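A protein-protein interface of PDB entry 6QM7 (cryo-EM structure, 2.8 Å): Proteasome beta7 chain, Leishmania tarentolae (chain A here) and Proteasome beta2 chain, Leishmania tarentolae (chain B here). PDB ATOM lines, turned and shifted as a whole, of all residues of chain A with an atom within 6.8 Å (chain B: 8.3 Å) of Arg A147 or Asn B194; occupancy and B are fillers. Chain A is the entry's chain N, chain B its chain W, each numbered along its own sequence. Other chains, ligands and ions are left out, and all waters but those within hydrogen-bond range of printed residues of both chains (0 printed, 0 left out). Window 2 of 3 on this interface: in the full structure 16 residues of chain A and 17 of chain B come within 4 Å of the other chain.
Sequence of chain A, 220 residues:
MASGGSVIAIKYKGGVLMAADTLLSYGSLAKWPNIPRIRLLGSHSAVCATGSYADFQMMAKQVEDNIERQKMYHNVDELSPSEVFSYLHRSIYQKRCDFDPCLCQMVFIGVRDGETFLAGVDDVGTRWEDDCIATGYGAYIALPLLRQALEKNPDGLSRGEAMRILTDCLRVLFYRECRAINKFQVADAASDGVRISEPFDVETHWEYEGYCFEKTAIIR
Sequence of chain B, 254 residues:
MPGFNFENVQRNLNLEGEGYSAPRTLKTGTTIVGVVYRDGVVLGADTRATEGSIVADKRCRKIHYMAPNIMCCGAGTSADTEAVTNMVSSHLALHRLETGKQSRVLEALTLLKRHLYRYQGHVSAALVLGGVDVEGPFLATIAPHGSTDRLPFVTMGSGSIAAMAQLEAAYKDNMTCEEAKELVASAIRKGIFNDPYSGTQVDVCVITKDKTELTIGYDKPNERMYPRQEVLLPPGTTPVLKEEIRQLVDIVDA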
ATOM      1  N   ILE A  10     -40.464 -11.790  13.866  1.00  0.00           N
ATOM      2  CA  ILE A  10     -39.876 -11.882  12.510  1.00  0.00           C
ATOM      3  C   ILE A  10     -40.948 -11.549  11.485  1.00  0.00           C
ATOM      4  O   ILE A  10     -42.068 -12.035  11.630  1.00  0.00           O
ATOM      5  CB  ILE A  10     -39.236 -13.263  12.288  1.00  0.00           C
ATOM      6  CG1 ILE A  10     -38.445 -13.307  10.985  1.00  0.00           C
ATOM      7  CG2 ILE A  10     -40.236 -14.399  12.351  1.00  0.00           C
ATOM      8  CD1 ILE A  10     -37.494 -14.484  10.908  1.00  0.00           C
ATOM      9  N   TRP A 128     -35.396   0.705  16.833  1.00  0.00           N
ATOM     10  CA  TRP A 128     -34.864   0.131  15.582  1.00  0.00           C
ATOM     11  C   TRP A 128     -35.939  -0.701  14.909  1.00  0.00           C
ATOM     12  O   TRP A 128     -36.608  -1.452  15.598  1.00  0.00           O
ATOM     13  CB  TRP A 128     -33.604  -0.667  15.879  1.00  0.00           C
ATOM     14  CG  TRP A 128     -33.809  -1.868  16.745  1.00  0.00           C
ATOM     15  CD1 TRP A 128     -33.957  -3.145  16.314  1.00  0.00           C
ATOM     16  CD2 TRP A 128     -33.848  -1.922  18.181  1.00  0.00           C
ATOM     17  NE1 TRP A 128     -34.120  -3.982  17.379  1.00  0.00           N
ATOM     18  CE2 TRP A 128     -34.055  -3.266  18.535  1.00  0.00           C
ATOM     19  CE3 TRP A 128     -33.749  -0.972  19.203  1.00  0.00           C
ATOM     20  CZ2 TRP A 128     -34.168  -3.688  19.856  1.00  0.00           C
ATOM     21  CZ3 TRP A 128     -33.857  -1.385  20.516  1.00  0.00           C
ATOM     22  CH2 TRP A 128     -34.069  -2.725  20.835  1.00  0.00           C
ATOM     23  N   ASP A 130     -36.520  -3.617  11.946  1.00  0.00           N
ATOM     24  CA  ASP A 130     -35.736  -4.688  11.288  1.00  0.00           C
ATOM     25  C   ASP A 130     -36.693  -5.770  10.817  1.00  0.00           C
ATOM     26  O   ASP A 130     -37.871  -5.678  11.159  1.00  0.00           O
ATOM     27  CB  ASP A 130     -34.669  -5.244  12.228  1.00  0.00           C
ATOM     28  CG  ASP A 130     -33.339  -5.510  11.543  1.00  0.00           C
ATOM     29  OD1 ASP A 130     -33.351  -6.205  10.493  1.00  0.00           O
ATOM     30  OD2 ASP A 130     -32.309  -5.004  12.049  1.00  0.00           O
ATOM     31  N   CYS A 132     -36.291  -8.836  11.686  1.00  0.00           N
ATOM     32  CA  CYS A 132     -36.452  -9.630  12.928  1.00  0.00           C
ATOM     33  C   CYS A 132     -35.929  -8.859  14.141  1.00  0.00           C
ATOM     34  O   CYS A 132     -34.847  -8.285  14.078  1.00  0.00           O
ATOM     35  CB  CYS A 132     -35.708 -10.948  12.822  1.00  0.00           C
ATOM     36  SG  CYS A 132     -33.918 -10.728  12.920  1.00  0.00           S
ATOM     37  N   ALA A 139     -32.414 -11.687  22.105  1.00  0.00           N
ATOM     38  CA  ALA A 139     -31.425 -10.869  21.384  1.00  0.00           C
ATOM     39  C   ALA A 139     -30.122 -11.643  21.223  1.00  0.00           C
ATOM     40  O   ALA A 139     -29.462 -11.478  20.188  1.00  0.00           O
ATOM     41  CB  ALA A 139     -31.198  -9.597  22.151  1.00  0.00           C
ATOM     42  N   TYR A 140     -29.753 -12.426  22.231  1.00  0.00           N
ATOM     43  CA  TYR A 140     -28.447 -13.117  22.320  1.00  0.00           C
ATOM     44  C   TYR A 140     -28.561 -14.502  21.702  1.00  0.00           C
ATOM     45  O   TYR A 140     -27.557 -14.970  21.159  1.00  0.00           O
ATOM     46  CB  TYR A 140     -27.994 -13.148  23.776  1.00  0.00           C
ATOM     47  CG  TYR A 140     -27.821 -11.766  24.353  1.00  0.00           C
ATOM     48  CD1 TYR A 140     -26.837 -10.916  23.870  1.00  0.00           C
ATOM     49  CD2 TYR A 140     -28.647 -11.295  25.361  1.00  0.00           C
ATOM     50  CE1 TYR A 140     -26.669  -9.639  24.383  1.00  0.00           C
ATOM     51  CE2 TYR A 140     -28.495 -10.018  25.883  1.00  0.00           C
ATOM     52  CZ  TYR A 140     -27.504  -9.184  25.390  1.00  0.00           C
ATOM     53  OH  TYR A 140     -27.344  -7.925  25.898  1.00  0.00           O
ATOM     54  N   ALA A 142     -31.900 -16.031  20.097  1.00  0.00           N
ATOM     55  CA  ALA A 142     -32.869 -16.209  19.003  1.00  0.00           C
ATOM     56  C   ALA A 142     -32.415 -15.384  17.811  1.00  0.00           C
ATOM     57  O   ALA A 142     -32.496 -15.901  16.699  1.00  0.00           O
ATOM     58  CB  ALA A 142     -34.260 -15.849  19.458  1.00  0.00           C
ATOM     59  N   LEU A 143     -31.959 -14.158  18.020  1.00  0.00           N
ATOM     60  CA  LEU A 143     -31.672 -13.252  16.876  1.00  0.00           C
ATOM     61  C   LEU A 143     -30.726 -13.919  15.889  1.00  0.00           C
ATOM     62  O   LEU A 143     -31.084 -14.050  14.723  1.00  0.00           O
ATOM     63  CB  LEU A 143     -31.088 -11.921  17.339  1.00  0.00           C
ATOM     64  CG  LEU A 143     -32.057 -10.753  17.369  1.00  0.00           C
ATOM     65  CD1 LEU A 143     -31.284  -9.458  17.571  1.00  0.00           C
ATOM     66  CD2 LEU A 143     -32.915 -10.704  16.114  1.00  0.00           C
ATOM     67  N   PRO A 144     -29.514 -14.352  16.302  1.00  0.00           N
ATOM     68  CA  PRO A 144     -28.614 -15.071  15.409  1.00  0.00           C
ATOM     69  C   PRO A 144     -29.324 -16.037  14.452  1.00  0.00           C
ATOM     70  O   PRO A 144     -29.027 -15.991  13.277  1.00  0.00           O
ATOM     71  CB  PRO A 144     -27.758 -15.849  16.411  1.00  0.00           C
ATOM     72  CG  PRO A 144     -27.595 -14.877  17.556  1.00  0.00           C
ATOM     73  CD  PRO A 144     -28.929 -14.168  17.640  1.00  0.00           C
ATOM     74  N   LEU A 145     -30.255 -16.838  14.975  1.00  0.00           N
ATOM     75  CA  LEU A 145     -30.981 -17.881  14.213  1.00  0.00           C
ATOM     76  C   LEU A 145     -31.977 -17.239  13.264  1.00  0.00           C
ATOM     77  O   LEU A 145     -32.068 -17.718  12.121  1.00  0.00           O
ATOM     78  CB  LEU A 145     -31.718 -18.818  15.167  1.00  0.00           C
ATOM     79  CG  LEU A 145     -30.850 -19.522  16.206  1.00  0.00           C
ATOM     80  CD1 LEU A 145     -31.661 -20.604  16.908  1.00  0.00           C
ATOM     81  CD2 LEU A 145     -29.601 -20.115  15.573  1.00  0.00           C
ATOM     82  N   LEU A 146     -32.737 -16.257  13.742  1.00  0.00           N
ATOM     83  CA  LEU A 146     -33.769 -15.568  12.928  1.00  0.00           C
ATOM     84  C   LEU A 146     -33.076 -14.868  11.769  1.00  0.00           C
ATOM     85  O   LEU A 146     -33.568 -14.977  10.654  1.00  0.00           O
ATOM     86  CB  LEU A 146     -34.514 -14.546  13.782  1.00  0.00           C
ATOM     87  CG  LEU A 146     -35.400 -15.122  14.875  1.00  0.00           C
ATOM     88  CD1 LEU A 146     -35.806 -14.037  15.855  1.00  0.00           C
ATOM     89  CD2 LEU A 146     -36.630 -15.782  14.277  1.00  0.00           C
ATOM     90  N   ARG A 147     -31.982 -14.170  12.056  1.00  0.00           N
ATOM     91  CA  ARG A 147     -31.197 -13.412  11.058  1.00  0.00           C
ATOM     92  C   ARG A 147     -30.672 -14.359   9.991  1.00  0.00           C
ATOM     93  O   ARG A 147     -30.726 -13.974   8.810  1.00  0.00           O
ATOM     94  CB  ARG A 147     -30.038 -12.682  11.726  1.00  0.00           C
ATOM     95  CG  ARG A 147     -30.489 -11.487  12.544  1.00  0.00           C
ATOM     96  CD  ARG A 147     -29.357 -10.499  12.604  1.00  0.00           C
ATOM     97  NE  ARG A 147     -29.724  -9.347  13.410  1.00  0.00           N
ATOM     98  CZ  ARG A 147     -29.250  -9.062  14.617  1.00  0.00           C
ATOM     99  NH1 ARG A 147     -28.353  -9.833  15.227  1.00  0.00           N
ATOM    100  NH2 ARG A 147     -29.690  -7.965  15.206  1.00  0.00           N
ATOM    101  N   GLN A 148     -30.171 -15.524  10.405  1.00  0.00           N
ATOM    102  CA  GLN A 148     -29.683 -16.593   9.499  1.00  0.00           C
ATOM    103  C   GLN A 148     -30.838 -17.030   8.597  1.00  0.00           C
ATOM    104  O   GLN A 148     -30.583 -17.237   7.409  1.00  0.00           O
ATOM    105  CB  GLN A 148     -29.099 -17.763  10.297  1.00  0.00           C
ATOM    106  CG  GLN A 148     -28.622 -18.942   9.450  1.00  0.00           C
ATOM    107  CD  GLN A 148     -28.183 -20.113  10.297  1.00  0.00           C
ATOM    108  OE1 GLN A 148     -27.044 -20.579  10.229  1.00  0.00           O
ATOM    109  NE2 GLN A 148     -29.085 -20.581  11.141  1.00  0.00           N
ATOM    110  N   ALA A 149     -32.052 -17.162   9.130  1.00  0.00           N
ATOM    111  CA  ALA A 149     -33.234 -17.616   8.357  1.00  0.00           C
ATOM    112  C   ALA A 149     -33.626 -16.565   7.320  1.00  0.00           C
ATOM    113  O   ALA A 149     -34.153 -16.966   6.275  1.00  0.00           O
ATOM    114  CB  ALA A 149     -34.395 -17.934   9.259  1.00  0.00           C
ATOM    115  N   LEU A 150     -33.385 -15.284   7.599  1.00  0.00           N
ATOM    116  CA  LEU A 150     -33.683 -14.156   6.678  1.00  0.00           C
ATOM    117  C   LEU A 150     -32.593 -14.038   5.609  1.00  0.00           C
ATOM    118  O   LEU A 150     -32.942 -13.682   4.475  1.00  0.00           O
ATOM    119  CB  LEU A 150     -33.786 -12.861   7.481  1.00  0.00           C
ATOM    120  CG  LEU A 150     -35.006 -12.752   8.389  1.00  0.00           C
ATOM    121  CD1 LEU A 150     -34.811 -11.628   9.394  1.00  0.00           C
ATOM    122  CD2 LEU A 150     -36.275 -12.541   7.582  1.00  0.00           C
ATOM    123  N   GLU A 151     -31.331 -14.279   5.973  1.00  0.00           N
ATOM    124  CA  GLU A 151     -30.149 -14.265   5.062  1.00  0.00           C
ATOM    125  C   GLU A 151     -30.304 -15.406   4.041  1.00  0.00           C
ATOM    126  O   GLU A 151     -29.967 -15.189   2.867  1.00  0.00           O
ATOM    127  CB  GLU A 151     -28.869 -14.275   5.919  1.00  0.00           C
ATOM    128  CG  GLU A 151     -27.684 -15.078   5.379  1.00  0.00           C
ATOM    129  CD  GLU A 151     -26.756 -15.664   6.444  1.00  0.00           C
ATOM    130  OE1 GLU A 151     -26.164 -14.875   7.222  1.00  0.00           O
ATOM    131  OE2 GLU A 151     -26.634 -16.916   6.508  1.00  0.00           O
ATOM    132  N   LYS A 152     -30.823 -16.563   4.466  1.00  0.00           N
ATOM    133  CA  LYS A 152     -30.998 -17.783   3.625  1.00  0.00           C
ATOM    134  C   LYS A 152     -32.183 -17.608   2.668  1.00  0.00           C
ATOM    135  O   LYS A 152     -32.126 -18.175   1.563  1.00  0.00           O
ATOM    136  CB  LYS A 152     -31.231 -19.025   4.496  1.00  0.00           C
ATOM    137  CG  LYS A 152     -30.232 -20.158   4.297  1.00  0.00           C
ATOM    138  CD  LYS A 152     -29.813 -20.848   5.587  1.00  0.00           C
ATOM    139  CE  LYS A 152     -28.372 -21.321   5.574  1.00  0.00           C
ATOM    140  NZ  LYS A 152     -27.861 -21.531   6.948  1.00  0.00           N
ATOM    141  N   ILE A 165     -39.094 -21.296  12.175  1.00  0.00           N
ATOM    142  CA  ILE A 165     -37.863 -20.680  12.750  1.00  0.00           C
ATOM    143  C   ILE A 165     -38.185 -20.066  14.122  1.00  0.00           C
ATOM    144  O   ILE A 165     -37.347 -20.240  15.022  1.00  0.00           O
ATOM    145  CB  ILE A 165     -37.144 -19.700  11.791  1.00  0.00           C
ATOM    146  CG1 ILE A 165     -35.776 -19.287  12.350  1.00  0.00           C
ATOM    147  CG2 ILE A 165     -37.974 -18.476  11.464  1.00  0.00           C
ATOM    148  CD1 ILE A 165     -34.807 -20.449  12.558  1.00  0.00           C
ATOM    149  N   THR B  31     -15.484 -16.587  20.045  1.00  0.00           N
ATOM    150  CA  THR B  31     -16.476 -17.683  20.050  1.00  0.00           C
ATOM    151  C   THR B  31     -15.740 -18.961  19.668  1.00  0.00           C
ATOM    152  O   THR B  31     -15.141 -18.987  18.595  1.00  0.00           O
ATOM    153  CB  THR B  31     -17.661 -17.428  19.118  1.00  0.00           C
ATOM    154  OG1 THR B  31     -18.428 -18.630  18.997  1.00  0.00           O
ATOM    155  CG2 THR B  31     -17.230 -17.002  17.740  1.00  0.00           C
ATOM    156  N   SER B 158     -17.273 -14.792  24.293  1.00  0.00           N
ATOM    157  CA  SER B 158     -18.266 -13.702  24.153  1.00  0.00           C
ATOM    158  C   SER B 158     -19.405 -14.164  23.252  1.00  0.00           C
ATOM    159  O   SER B 158     -20.552 -13.856  23.586  1.00  0.00           O
ATOM    160  CB  SER B 158     -17.598 -12.464  23.607  1.00  0.00           C
ATOM    161  OG  SER B 158     -16.184 -12.514  23.796  1.00  0.00           O
ATOM    162  N   GLY B 159     -19.100 -14.873  22.164  1.00  0.00           N
ATOM    163  CA  GLY B 159     -20.110 -15.347  21.194  1.00  0.00           C
ATOM    164  C   GLY B 159     -20.623 -16.746  21.516  1.00  0.00           C
ATOM    165  O   GLY B 159     -21.237 -17.367  20.634  1.00  0.00           O
ATOM    166  N   ILE B 161     -23.120 -17.685  23.380  1.00  0.00           N
ATOM    167  CA  ILE B 161     -24.600 -17.796  23.484  1.00  0.00           C
ATOM    168  C   ILE B 161     -25.190 -17.866  22.072  1.00  0.00           C
ATOM    169  O   ILE B 161     -26.024 -18.745  21.816  1.00  0.00           O
ATOM    170  CB  ILE B 161     -25.157 -16.643  24.328  1.00  0.00           C
ATOM    171  CG1 ILE B 161     -24.646 -16.740  25.766  1.00  0.00           C
ATOM    172  CG2 ILE B 161     -26.670 -16.623  24.249  1.00  0.00           C
ATOM    173  CD1 ILE B 161     -25.219 -15.712  26.718  1.00  0.00           C
ATOM    174  N   ALA B 162     -24.748 -16.989  21.185  1.00  0.00           N
ATOM    175  CA  ALA B 162     -25.132 -16.993  19.758  1.00  0.00           C
ATOM    176  C   ALA B 162     -24.802 -18.356  19.156  1.00  0.00           C
ATOM    177  O   ALA B 162     -25.694 -18.937  18.518  1.00  0.00           O
ATOM    178  CB  ALA B 162     -24.418 -15.887  19.023  1.00  0.00           C
ATOM    179  N   ALA B 163     -23.574 -18.832  19.361  1.00  0.00           N
ATOM    180  CA  ALA B 163     -23.070 -20.104  18.806  1.00  0.00           C
ATOM    181  C   ALA B 163     -23.918 -21.247  19.329  1.00  0.00           C
ATOM    182  O   ALA B 163     -24.353 -22.068  18.514  1.00  0.00           O
ATOM    183  CB  ALA B 163     -21.637 -20.318  19.185  1.00  0.00           C
ATOM    184  N   SER B 186     -21.199 -23.098  11.188  1.00  0.00           N
ATOM    185  CA  SER B 186     -22.481 -22.354  11.329  1.00  0.00           C
ATOM    186  C   SER B 186     -22.536 -21.688  12.701  1.00  0.00           C
ATOM    187  O   SER B 186     -22.918 -20.536  12.773  1.00  0.00           O
ATOM    188  CB  SER B 186     -23.675 -23.273  11.122  1.00  0.00           C
ATOM    189  OG  SER B 186     -24.896 -22.545  11.052  1.00  0.00           O
ATOM    190  N   ALA B 187     -22.191 -22.430  13.750  1.00  0.00           N
ATOM    191  CA  ALA B 187     -22.184 -21.965  15.156  1.00  0.00           C
ATOM    192  C   ALA B 187     -21.206 -20.806  15.295  1.00  0.00           C
ATOM    193  O   ALA B 187     -21.562 -19.821  15.927  1.00  0.00           O
ATOM    194  CB  ALA B 187     -21.806 -23.087  16.085  1.00  0.00           C
ATOM    195  N   ILE B 188     -20.000 -20.948  14.754  1.00  0.00           N
ATOM    196  CA  ILE B 188     -18.942 -19.910  14.857  1.00  0.00           C
ATOM    197  C   ILE B 188     -19.449 -18.681  14.129  1.00  0.00           C
ATOM    198  O   ILE B 188     -19.409 -17.614  14.734  1.00  0.00           O
ATOM    199  CB  ILE B 188     -17.607 -20.394  14.281  1.00  0.00           C
ATOM    200  CG1 ILE B 188     -17.027 -21.537  15.119  1.00  0.00           C
ATOM    201  CG2 ILE B 188     -16.625 -19.228  14.163  1.00  0.00           C
ATOM    202  CD1 ILE B 188     -16.789 -21.160  16.569  1.00  0.00           C
ATOM    203  N   ARG B 189     -19.932 -18.844  12.903  1.00  0.00           N
ATOM    204  CA  ARG B 189     -20.500 -17.734  12.112  1.00  0.00           C
ATOM    205  C   ARG B 189     -21.490 -16.959  12.981  1.00  0.00           C
ATOM    206  O   ARG B 189     -21.414 -15.731  12.959  1.00  0.00           O
ATOM    207  CB  ARG B 189     -21.133 -18.226  10.811  1.00  0.00           C
ATOM    208  CG  ARG B 189     -20.120 -18.486   9.703  1.00  0.00           C
ATOM    209  CD  ARG B 189     -20.757 -18.435   8.323  1.00  0.00           C
ATOM    210  NE  ARG B 189     -21.874 -19.358   8.278  1.00  0.00           N
ATOM    211  CZ  ARG B 189     -21.780 -20.682   8.166  1.00  0.00           C
ATOM    212  NH1 ARG B 189     -22.887 -21.410   8.164  1.00  0.00           N
ATOM    213  NH2 ARG B 189     -20.606 -21.286   8.061  1.00  0.00           N
ATOM    214  N   LYS B 190     -22.349 -17.612  13.757  1.00  0.00           N
ATOM    215  CA  LYS B 190     -23.300 -16.888  14.645  1.00  0.00           C
ATOM    216  C   LYS B 190     -22.536 -15.907  15.530  1.00  0.00           C
ATOM    217  O   LYS B 190     -22.998 -14.783  15.694  1.00  0.00           O
ATOM    218  CB  LYS B 190     -24.085 -17.802  15.593  1.00  0.00           C
ATOM    219  CG  LYS B 190     -24.997 -18.808  14.922  1.00  0.00           C
ATOM    220  CD  LYS B 190     -26.071 -18.207  14.061  1.00  0.00           C
ATOM    221  CE  LYS B 190     -26.306 -19.015  12.805  1.00  0.00           C
ATOM    222  NZ  LYS B 190     -25.180 -18.909  11.847  1.00  0.00           N
ATOM    223  N   GLY B 191     -21.440 -16.356  16.128  1.00  0.00           N
ATOM    224  CA  GLY B 191     -20.574 -15.488  16.937  1.00  0.00           C
ATOM    225  C   GLY B 191     -19.977 -14.393  16.073  1.00  0.00           C
ATOM    226  O   GLY B 191     -20.141 -13.224  16.415  1.00  0.00           O
ATOM    227  N   ILE B 192     -19.340 -14.769  14.970  1.00  0.00           N
ATOM    228  CA  ILE B 192     -18.663 -13.825  14.043  1.00  0.00           C
ATOM    229  C   ILE B 192     -19.579 -12.625  13.799  1.00  0.00           C
ATOM    230  O   ILE B 192     -19.155 -11.478  14.136  1.00  0.00           O
ATOM    231  CB  ILE B 192     -18.260 -14.537  12.744  1.00  0.00           C
ATOM    232  CG1 ILE B 192     -17.000 -15.371  12.979  1.00  0.00           C
ATOM    233  CG2 ILE B 192     -18.089 -13.553  11.599  1.00  0.00           C
ATOM    234  CD1 ILE B 192     -16.577 -16.179  11.786  1.00  0.00           C
ATOM    235  N   PHE B 193     -20.785 -12.888  13.296  1.00  0.00           N
ATOM    236  CA  PHE B 193     -21.712 -11.866  12.747  1.00  0.00           C
ATOM    237  C   PHE B 193     -22.487 -11.137  13.844  1.00  0.00           C
ATOM    238  O   PHE B 193     -22.849  -9.987  13.601  1.00  0.00           O
ATOM    239  CB  PHE B 193     -22.673 -12.507  11.752  1.00  0.00           C
ATOM    240  CG  PHE B 193     -21.993 -12.891  10.469  1.00  0.00           C
ATOM    241  CD1 PHE B 193     -21.349 -11.929   9.707  1.00  0.00           C
ATOM    242  CD2 PHE B 193     -21.963 -14.204  10.038  1.00  0.00           C
ATOM    243  CE1 PHE B 193     -20.698 -12.266   8.532  1.00  0.00           C
ATOM    244  CE2 PHE B 193     -21.305 -14.543   8.865  1.00  0.00           C
ATOM    245  CZ  PHE B 193     -20.679 -13.573   8.116  1.00  0.00           C
ATOM    246  N   ASN B 194     -22.749 -11.771  14.984  1.00  0.00           N
ATOM    247  CA  ASN B 194     -23.705 -11.258  15.996  1.00  0.00           C
ATOM    248  C   ASN B 194     -22.979 -10.830  17.274  1.00  0.00           C
ATOM    249  O   ASN B 194     -23.627 -10.139  18.089  1.00  0.00           O
ATOM    250  CB  ASN B 194     -24.828 -12.267  16.243  1.00  0.00           C
ATOM    251  CG  ASN B 194     -25.527 -12.675  14.960  1.00  0.00           C
ATOM    252  OD1 ASN B 194     -26.146 -11.849  14.292  1.00  0.00           O
ATOM    253  ND2 ASN B 194     -25.420 -13.940  14.591  1.00  0.00           N
ATOM    254  N   ASP B 195     -21.711 -11.203  17.453  1.00  0.00           N
ATOM    255  CA  ASP B 195     -20.833 -10.737  18.559  1.00  0.00           C
ATOM    256  C   ASP B 195     -19.754  -9.839  17.959  1.00  0.00           C
ATOM    257  O   ASP B 195     -19.172 -10.149  16.908  1.00  0.00           O
ATOM    258  CB  ASP B 195     -20.254 -11.921  19.343  1.00  0.00           C
ATOM    259  CG  ASP B 195     -19.063 -11.617  20.251  1.00  0.00           C
ATOM    260  OD1 ASP B 195     -19.122 -10.612  20.986  1.00  0.00           O
ATOM    261  OD2 ASP B 195     -18.087 -12.414  20.248  1.00  0.00           O
ATOM    262  N   PRO B 196     -19.492  -8.669  18.586  1.00  0.00           N
ATOM    263  CA  PRO B 196     -18.418  -7.782  18.140  1.00  0.00           C
ATOM    264  C   PRO B 196     -16.992  -8.267  18.445  1.00  0.00           C
ATOM    265  O   PRO B 196     -16.111  -7.938  17.683  1.00  0.00           O
ATOM    266  CB  PRO B 196     -18.728  -6.487  18.892  1.00  0.00           C
ATOM    267  CG  PRO B 196     -19.384  -6.962  20.161  1.00  0.00           C
ATOM    268  CD  PRO B 196     -20.279  -8.079  19.684  1.00  0.00           C
ATOM    269  N   TYR B 197     -16.779  -9.032  19.508  1.00  0.00           N
ATOM    270  CA  TYR B 197     -15.431  -9.542  19.880  1.00  0.00           C
ATOM    271  C   TYR B 197     -15.031 -10.754  19.030  1.00  0.00           C
ATOM    272  O   TYR B 197     -13.830 -11.080  19.016  1.00  0.00           O
ATOM    273  CB  TYR B 197     -15.372  -9.829  21.379  1.00  0.00           C
ATOM    274  CG  TYR B 197     -15.458  -8.557  22.174  1.00  0.00           C
ATOM    275  CD1 TYR B 197     -14.353  -7.730  22.282  1.00  0.00           C
ATOM    276  CD2 TYR B 197     -16.652  -8.126  22.728  1.00  0.00           C
ATOM    277  CE1 TYR B 197     -14.418  -6.528  22.966  1.00  0.00           C
ATOM    278  CE2 TYR B 197     -16.735  -6.923  23.414  1.00  0.00           C
ATOM    279  CZ  TYR B 197     -15.612  -6.121  23.536  1.00  0.00           C
ATOM    280  OH  TYR B 197     -15.675  -4.935  24.211  1.00  0.00           O
ATOM    281  N   SER B 198     -15.983 -11.400  18.356  1.00  0.00           N
ATOM    282  CA  SER B 198     -15.742 -12.539  17.437  1.00  0.00           C
ATOM    283  C   SER B 198     -15.759 -12.010  16.015  1.00  0.00           C
ATOM    284  O   SER B 198     -16.571 -11.113  15.755  1.00  0.00           O
ATOM    285  CB  SER B 198     -16.776 -13.622  17.591  1.00  0.00           C
ATOM    286  OG  SER B 198     -16.826 -14.133  18.916  1.00  0.00           O
ATOM    287  N   GLY B 199     -14.942 -12.576  15.130  1.00  0.00           N
ATOM    288  CA  GLY B 199     -14.916 -12.120  13.736  1.00  0.00           C
ATOM    289  C   GLY B 199     -13.987 -12.902  12.843  1.00  0.00           C
ATOM    290  O   GLY B 199     -13.271 -13.788  13.340  1.00  0.00           O
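O of Tyr A140 sits close to N of Ala B162. The guanidinium group of Arg A147 lies within hydrogen-bond range of the side-chain amide oxygen of Asn B194 (3.1 Å). The side-chain amide oxygen of Gln A148 is in hydrogen-bond range of the side-chain hydroxyl of Ser B186, at 3.0 Å. The side-chain amide oxygen (OE1) of Gln A148 sits at hydrogen-bond distance from the side-chain amino group (NZ) of Lys B190.
The backbone carbonyl oxygen (O) of Ser B186 sits at hydrogen-bond distance from the side-chain amino group (NZ) of Lys B190, at 2.9 Å. O of Lys B190 is in hydrogen-bond range of ND2 of Asn B194, 2.8 Å away.
Ile B161 touches Tyr A140 (CG2 to O, 3.6 Å). Ala B162 touches Pro A144. Lys B190 touches Pro A144 (CD to CB, 3.7 Å). Asn B194 touches Pro A144.
Of the printed residues of chain B, Gln A148 touches Ser B186 (3.0 Å) and Lys B190 (3.0 Å). Lys A152 touches none of the printed residues of chain B. Of the printed residues of chain A, Ile B161 touches Tyr A140. Of the printed residues of chain A, Ser B186 touches Gln A148 (3.0 Å). Printed residues of chain A within 4 Å of Lys B190: Pro A144 (3.7 Å) and Gln A148 (3.0 Å). The nearest residue of chain A that does not touch Asn B194 is Leu A143 (5.3 Å).
Along chain B the printed residues that touch a printed residue of chain A span positions 161 to 194. Of the 18 printed residues of chain A, 4 touch a printed residue of chain B. Hydrophobic or aromatic side chains of chain A within 4 Å of the printed part of chain B: Tyr A140 and Pro A144. Among the printed residues, 8 pairs touch across the chains.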
